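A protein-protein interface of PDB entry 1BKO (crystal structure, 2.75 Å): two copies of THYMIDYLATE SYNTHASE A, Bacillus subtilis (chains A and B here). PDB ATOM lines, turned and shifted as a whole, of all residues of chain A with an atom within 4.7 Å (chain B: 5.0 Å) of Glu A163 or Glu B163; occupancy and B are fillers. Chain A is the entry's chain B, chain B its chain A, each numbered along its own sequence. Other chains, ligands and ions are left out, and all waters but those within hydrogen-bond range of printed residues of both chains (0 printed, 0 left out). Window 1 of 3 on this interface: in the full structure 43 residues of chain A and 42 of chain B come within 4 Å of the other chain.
OE1 of Glu B163 lies close to OE1 of Glu A163 (2.9 Å). The side-chain carboxylate of Glu B163 is in hydrogen-bond range of the side-chain hydroxyl of Tyr A162, at 2.8 Å. OH of Tyr B162 is in hydrogen-bond range of OE1 of Glu A163, at 3.4 Å. NH2 of Arg B178 is in hydrogen-bond range of OE1 of Gln A165 (3.4 Å). The side-chain amide oxygen (OE1) of Gln B165 is in hydrogen-bond range of the guanidinium group (NH1) of Arg A178. The side-chain carboxylate (OE2) of Glu A163 lies within salt-bridge range of the guanidinium group (NH1) of Arg B178 (3.8 Å). The side-chain carboxylate (OE2) of Glu A176 lies within salt-bridge range of the guanidinium group (NH2) of Arg B178. The side-chain carboxylate (OE2) of Glu B176 lies within salt-bridge range of the guanidinium group (NH2) of Arg A178 (3.1 Å).
Along chain A the printed residues that touch a printed residue of chain B span positions 145 to 178. Among the printed residues, 10 pairs touch across the chains. Among the printed residues, Asp or Glu carboxylates within 4 Å of a Lys or Arg side-chain nitrogen of the other chain: Glu A163 with Arg B178, Glu A176 with Arg B178 and Arg A178 with Glu B176.
Tyr A162 touches Glu B163, and with the chains exchanged Glu A163 touches Tyr B162. Glu B163 touches its own counterpart, Glu A163. Gln A165 touches Arg B178, and with the chains exchanged Arg A178 touches Gln B165. Glu A176 touches Arg B178, and with the chains exchanged Arg A178 touches Glu B176. Positions printed for both chains: 144, 145, 161, 162, 163, 164, 165, 176, 177 and 178.
Among the printed residues, pairs that only touch across the chains: Met A145 with Met B145 and Arg A178 with Glu B163.
Of chain B, only Tyr B162 (3.4 Å), Glu B163 (2.9 Å) and Arg B178 (3.8 Å) come within 4 Å of Glu A163. Of the printed residues of chain B, Gln A165 touches Arg B178. Glu B163 touches just these residues of chain A: Tyr A162 (2.8 Å), Glu A163 (2.9 Å) and Arg A178 (3.9 Å). Printed residues of chain A within 4 Å of Glu B176: Arg A178. The nearest printed residue of chain A that does not touch Glu B176 is Tyr A162 (6.9 Å).
OH of Tyr A162 lies within hydrogen-bond range of NH1 of Arg A178, at 2.6 Å. N of Gln B165 sits at hydrogen-bond distance from O of Glu B176, 2.9 Å away. The backbone carbonyl oxygen (O) of Glu B163 sits at hydrogen-bond distance from the backbone NH (N) of Arg B178. OH of Tyr B162 sits at hydrogen-bond distance from NH1 of Arg B178. The backbone carbonyl oxygen (O) of Gln A165 lies within hydrogen-bond range of the backbone NH (N) of Glu A176 (3.1 Å). O of Glu A163 lies within hydrogen-bond range of N of Arg A178, 3.4 Å away.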
ATOM      1  N   THR A 144      20.167  14.712   9.163  1.00  0.00           N
ATOM      2  CA  THR A 144      19.693  13.436   9.712  1.00  0.00           C
ATOM      3  C   THR A 144      18.728  12.797   8.717  1.00  0.00           C
ATOM      4  O   THR A 144      17.833  13.471   8.189  1.00  0.00           O
ATOM      5  CB  THR A 144      19.010  13.573  11.073  1.00  0.00           C
ATOM      6  OG1 THR A 144      18.794  14.955  11.387  1.00  0.00           O
ATOM      7  CG2 THR A 144      19.873  12.923  12.141  1.00  0.00           C
ATOM      8  N   MET A 145      18.918  11.505   8.447  1.00  0.00           N
ATOM      9  CA  MET A 145      18.089  10.803   7.470  1.00  0.00           C
ATOM     10  C   MET A 145      17.289   9.627   8.011  1.00  0.00           C
ATOM     11  O   MET A 145      17.851   8.675   8.562  1.00  0.00           O
ATOM     12  CB  MET A 145      18.961  10.324   6.298  1.00  0.00           C
ATOM     13  CG  MET A 145      18.189   9.883   5.060  1.00  0.00           C
ATOM     14  SD  MET A 145      17.080  11.189   4.500  1.00  0.00           S
ATOM     15  CE  MET A 145      18.230  12.383   3.930  1.00  0.00           C
ATOM     16  N   VAL A 161       7.956  13.115   8.406  1.00  0.00           N
ATOM     17  CA  VAL A 161       9.081  13.994   8.721  1.00  0.00           C
ATOM     18  C   VAL A 161      10.342  13.129   8.708  1.00  0.00           C
ATOM     19  O   VAL A 161      10.793  12.640   9.750  1.00  0.00           O
ATOM     20  CB  VAL A 161       8.911  14.617  10.120  1.00  0.00           C
ATOM     21  CG1 VAL A 161       9.793  15.825  10.253  1.00  0.00           C
ATOM     22  CG2 VAL A 161       7.465  14.985  10.372  1.00  0.00           C
ATOM     23  N   TYR A 162      10.903  12.945   7.519  1.00  0.00           N
ATOM     24  CA  TYR A 162      12.080  12.096   7.329  1.00  0.00           C
ATOM     25  C   TYR A 162      13.472  12.744   7.398  1.00  0.00           C
ATOM     26  O   TYR A 162      14.487  12.035   7.362  1.00  0.00           O
ATOM     27  CB  TYR A 162      11.950  11.371   5.989  1.00  0.00           C
ATOM     28  CG  TYR A 162      12.027  12.303   4.798  1.00  0.00           C
ATOM     29  CD1 TYR A 162      11.074  13.308   4.606  1.00  0.00           C
ATOM     30  CD2 TYR A 162      13.078  12.209   3.885  1.00  0.00           C
ATOM     31  CE1 TYR A 162      11.173  14.202   3.535  1.00  0.00           C
ATOM     32  CE2 TYR A 162      13.182  13.092   2.812  1.00  0.00           C
ATOM     33  CZ  TYR A 162      12.232  14.089   2.646  1.00  0.00           C
ATOM     34  OH  TYR A 162      12.372  14.990   1.621  1.00  0.00           O
ATOM     35  N   GLU A 163      13.542  14.069   7.467  1.00  0.00           N
ATOM     36  CA  GLU A 163      14.847  14.706   7.492  1.00  0.00           C
ATOM     37  C   GLU A 163      14.953  16.097   8.091  1.00  0.00           C
ATOM     38  O   GLU A 163      13.977  16.851   8.191  1.00  0.00           O
ATOM     39  CB  GLU A 163      15.419  14.748   6.078  1.00  0.00           C
ATOM     40  CG  GLU A 163      14.650  15.655   5.128  1.00  0.00           C
ATOM     41  CD  GLU A 163      15.379  15.885   3.815  1.00  0.00           C
ATOM     42  OE1 GLU A 163      16.393  15.191   3.548  1.00  0.00           O
ATOM     43  OE2 GLU A 163      14.936  16.764   3.046  1.00  0.00           O
ATOM     44  N   THR A 164      16.195  16.458   8.380  1.00  0.00           N
ATOM     45  CA  THR A 164      16.530  17.745   8.953  1.00  0.00           C
ATOM     46  C   THR A 164      17.988  18.093   8.693  1.00  0.00           C
ATOM     47  O   THR A 164      18.843  17.207   8.587  1.00  0.00           O
ATOM     48  CB  THR A 164      16.306  17.751  10.477  1.00  0.00           C
ATOM     49  OG1 THR A 164      16.447  16.420  10.989  1.00  0.00           O
ATOM     50  CG2 THR A 164      14.932  18.282  10.812  1.00  0.00           C
ATOM     51  N   GLN A 165      18.249  19.375   8.478  1.00  0.00           N
ATOM     52  CA  GLN A 165      19.610  19.846   8.292  1.00  0.00           C
ATOM     53  C   GLN A 165      19.785  21.013   9.236  1.00  0.00           C
ATOM     54  O   GLN A 165      18.942  21.917   9.284  1.00  0.00           O
ATOM     55  CB  GLN A 165      19.905  20.283   6.852  1.00  0.00           C
ATOM     56  CG  GLN A 165      21.343  20.804   6.687  1.00  0.00           C
ATOM     57  CD  GLN A 165      21.767  21.007   5.246  1.00  0.00           C
ATOM     58  OE1 GLN A 165      21.182  20.438   4.324  1.00  0.00           O
ATOM     59  NE2 GLN A 165      22.821  21.790   5.048  1.00  0.00           N
ATOM     60  N   GLU A 176      16.092  23.194   9.565  1.00  0.00           N
ATOM     61  CA  GLU A 176      15.189  23.104   8.411  1.00  0.00           C
ATOM     62  C   GLU A 176      14.577  21.693   8.462  1.00  0.00           C
ATOM     63  O   GLU A 176      15.294  20.704   8.678  1.00  0.00           O
ATOM     64  CB  GLU A 176      15.972  23.329   7.091  1.00  0.00           C
ATOM     65  CG  GLU A 176      15.112  23.563   5.823  1.00  0.00           C
ATOM     66  CD  GLU A 176      15.928  23.977   4.566  1.00  0.00           C
ATOM     67  OE1 GLU A 176      16.737  24.931   4.642  1.00  0.00           O
ATOM     68  OE2 GLU A 176      15.740  23.367   3.487  1.00  0.00           O
ATOM     69  N   VAL A 177      13.255  21.603   8.318  1.00  0.00           N
ATOM     70  CA  VAL A 177      12.577  20.314   8.367  1.00  0.00           C
ATOM     71  C   VAL A 177      11.713  20.080   7.126  1.00  0.00           C
ATOM     72  O   VAL A 177      10.970  20.971   6.707  1.00  0.00           O
ATOM     73  CB  VAL A 177      11.654  20.222   9.607  1.00  0.00           C
ATOM     74  CG1 VAL A 177      11.308  18.771   9.906  1.00  0.00           C
ATOM     75  CG2 VAL A 177      12.295  20.903  10.814  1.00  0.00           C
ATOM     76  N   ARG A 178      11.798  18.873   6.560  1.00  0.00           N
ATOM     77  CA  ARG A 178      11.003  18.516   5.378  1.00  0.00           C
ATOM     78  C   ARG A 178      10.250  17.201   5.557  1.00  0.00           C
ATOM     79  O   ARG A 178      10.834  16.165   5.899  1.00  0.00           O
ATOM     80  CB  ARG A 178      11.871  18.424   4.109  1.00  0.00           C
ATOM     81  CG  ARG A 178      11.057  18.226   2.808  1.00  0.00           C
ATOM     82  CD  ARG A 178      11.939  18.262   1.552  1.00  0.00           C
ATOM     83  NE  ARG A 178      11.184  18.335   0.292  1.00  0.00           N
ATOM     84  CZ  ARG A 178      10.494  17.327  -0.242  1.00  0.00           C
ATOM     85  NH1 ARG A 178      10.444  16.151   0.367  1.00  0.00           N
ATOM     86  NH2 ARG A 178       9.869  17.481  -1.401  1.00  0.00           N
ATOM     87  N   THR B 144      13.563   9.825  -4.563  1.00  0.00           N
ATOM     88  CA  THR B 144      14.868   9.298  -4.931  1.00  0.00           C
ATOM     89  C   THR B 144      15.790   9.824  -3.828  1.00  0.00           C
ATOM     90  O   THR B 144      15.671  10.986  -3.420  1.00  0.00           O
ATOM     91  CB  THR B 144      15.324   9.828  -6.302  1.00  0.00           C
ATOM     92  OG1 THR B 144      14.224   9.811  -7.225  1.00  0.00           O
ATOM     93  CG2 THR B 144      16.421   8.956  -6.859  1.00  0.00           C
ATOM     94  N   MET B 145      16.671   8.972  -3.311  1.00  0.00           N
ATOM     95  CA  MET B 145      17.566   9.375  -2.227  1.00  0.00           C
ATOM     96  C   MET B 145      18.999   8.869  -2.375  1.00  0.00           C
ATOM     97  O   MET B 145      19.263   7.681  -2.196  1.00  0.00           O
ATOM     98  CB  MET B 145      17.006   8.879  -0.888  1.00  0.00           C
ATOM     99  CG  MET B 145      17.905   9.136   0.321  1.00  0.00           C
ATOM    100  SD  MET B 145      17.936  10.875   0.762  1.00  0.00           S
ATOM    101  CE  MET B 145      16.176  11.170   0.965  1.00  0.00           C
ATOM    102  N   VAL B 161      23.260  17.907  -4.784  1.00  0.00           N
ATOM    103  CA  VAL B 161      21.891  17.645  -5.230  1.00  0.00           C
ATOM    104  C   VAL B 161      21.698  16.151  -4.962  1.00  0.00           C
ATOM    105  O   VAL B 161      22.027  15.311  -5.799  1.00  0.00           O
ATOM    106  CB  VAL B 161      21.735  17.965  -6.738  1.00  0.00           C
ATOM    107  CG1 VAL B 161      20.464  17.330  -7.296  1.00  0.00           C
ATOM    108  CG2 VAL B 161      21.700  19.483  -6.946  1.00  0.00           C
ATOM    109  N   TYR B 162      21.199  15.832  -3.772  1.00  0.00           N
ATOM    110  CA  TYR B 162      21.031  14.444  -3.341  1.00  0.00           C
ATOM    111  C   TYR B 162      19.641  13.794  -3.412  1.00  0.00           C
ATOM    112  O   TYR B 162      19.538  12.567  -3.494  1.00  0.00           O
ATOM    113  CB  TYR B 162      21.587  14.298  -1.923  1.00  0.00           C
ATOM    114  CG  TYR B 162      20.805  15.085  -0.900  1.00  0.00           C
ATOM    115  CD1 TYR B 162      20.786  16.483  -0.924  1.00  0.00           C
ATOM    116  CD2 TYR B 162      20.040  14.432   0.066  1.00  0.00           C
ATOM    117  CE1 TYR B 162      20.018  17.205  -0.018  1.00  0.00           C
ATOM    118  CE2 TYR B 162      19.272  15.144   0.975  1.00  0.00           C
ATOM    119  CZ  TYR B 162      19.258  16.528   0.926  1.00  0.00           C
ATOM    120  OH  TYR B 162      18.444  17.220   1.792  1.00  0.00           O
ATOM    121  N   GLU B 163      18.573  14.580  -3.358  1.00  0.00           N
ATOM    122  CA  GLU B 163      17.251  13.971  -3.402  1.00  0.00           C
ATOM    123  C   GLU B 163      16.222  14.651  -4.290  1.00  0.00           C
ATOM    124  O   GLU B 163      16.266  15.868  -4.525  1.00  0.00           O
ATOM    125  CB  GLU B 163      16.672  13.859  -1.998  1.00  0.00           C
ATOM    126  CG  GLU B 163      16.331  15.204  -1.396  1.00  0.00           C
ATOM    127  CD  GLU B 163      15.557  15.093  -0.108  1.00  0.00           C
ATOM    128  OE1 GLU B 163      15.966  14.297   0.772  1.00  0.00           O
ATOM    129  OE2 GLU B 163      14.543  15.816   0.023  1.00  0.00           O
ATOM    130  N   THR B 164      15.242  13.847  -4.695  1.00  0.00           N
ATOM    131  CA  THR B 164      14.150  14.290  -5.541  1.00  0.00           C
ATOM    132  C   THR B 164      12.828  13.706  -5.091  1.00  0.00           C
ATOM    133  O   THR B 164      12.773  12.639  -4.468  1.00  0.00           O
ATOM    134  CB  THR B 164      14.355  13.876  -7.004  1.00  0.00           C
ATOM    135  OG1 THR B 164      14.891  12.549  -7.061  1.00  0.00           O
ATOM    136  CG2 THR B 164      15.298  14.835  -7.703  1.00  0.00           C
ATOM    137  N   GLN B 165      11.768  14.460  -5.353  1.00  0.00           N
ATOM    138  CA  GLN B 165      10.417  14.033  -5.035  1.00  0.00           C
ATOM    139  C   GLN B 165       9.526  14.433  -6.192  1.00  0.00           C
ATOM    140  O   GLN B 165       9.369  15.615  -6.482  1.00  0.00           O
ATOM    141  CB  GLN B 165       9.909  14.662  -3.743  1.00  0.00           C
ATOM    142  CG  GLN B 165       8.429  14.418  -3.539  1.00  0.00           C
ATOM    143  CD  GLN B 165       8.057  14.078  -2.116  1.00  0.00           C
ATOM    144  OE1 GLN B 165       8.915  13.858  -1.258  1.00  0.00           O
ATOM    145  NE2 GLN B 165       6.763  13.985  -1.866  1.00  0.00           N
ATOM    146  N   GLU B 176      10.621  18.195  -7.755  1.00  0.00           N
ATOM    147  CA  GLU B 176      11.200  19.035  -6.703  1.00  0.00           C
ATOM    148  C   GLU B 176      12.536  18.374  -6.328  1.00  0.00           C
ATOM    149  O   GLU B 176      12.582  17.167  -6.063  1.00  0.00           O
ATOM    150  CB  GLU B 176      10.278  19.125  -5.465  1.00  0.00           C
ATOM    151  CG  GLU B 176      10.912  19.829  -4.231  1.00  0.00           C
ATOM    152  CD  GLU B 176       9.900  20.245  -3.141  1.00  0.00           C
ATOM    153  OE1 GLU B 176       8.681  20.329  -3.418  1.00  0.00           O
ATOM    154  OE2 GLU B 176      10.328  20.506  -1.991  1.00  0.00           O
ATOM    155  N   VAL B 177      13.625  19.141  -6.379  1.00  0.00           N
ATOM    156  CA  VAL B 177      14.948  18.618  -6.034  1.00  0.00           C
ATOM    157  C   VAL B 177      15.529  19.386  -4.847  1.00  0.00           C
ATOM    158  O   VAL B 177      15.298  20.597  -4.713  1.00  0.00           O
ATOM    159  CB  VAL B 177      15.949  18.755  -7.207  1.00  0.00           C
ATOM    160  CG1 VAL B 177      17.215  17.977  -6.900  1.00  0.00           C
ATOM    161  CG2 VAL B 177      15.329  18.286  -8.514  1.00  0.00           C
ATOM    162  N   ARG B 178      16.289  18.685  -4.002  1.00  0.00           N
ATOM    163  CA  ARG B 178      16.917  19.305  -2.835  1.00  0.00           C
ATOM    164  C   ARG B 178      18.438  19.286  -2.904  1.00  0.00           C
ATOM    165  O   ARG B 178      19.062  18.244  -3.127  1.00  0.00           O
ATOM    166  CB  ARG B 178      16.485  18.632  -1.532  1.00  0.00           C
ATOM    167  CG  ARG B 178      17.128  19.236  -0.274  1.00  0.00           C
ATOM    168  CD  ARG B 178      16.336  20.411   0.267  1.00  0.00           C
ATOM    169  NE  ARG B 178      17.086  21.251   1.206  1.00  0.00           N
ATOM    170  CZ  ARG B 178      17.592  20.858   2.376  1.00  0.00           C
ATOM    171  NH1 ARG B 178      17.448  19.610   2.803  1.00  0.00           N
ATOM    172  NH2 ARG B 178      18.253  21.727   3.131  1.00  0.00           N
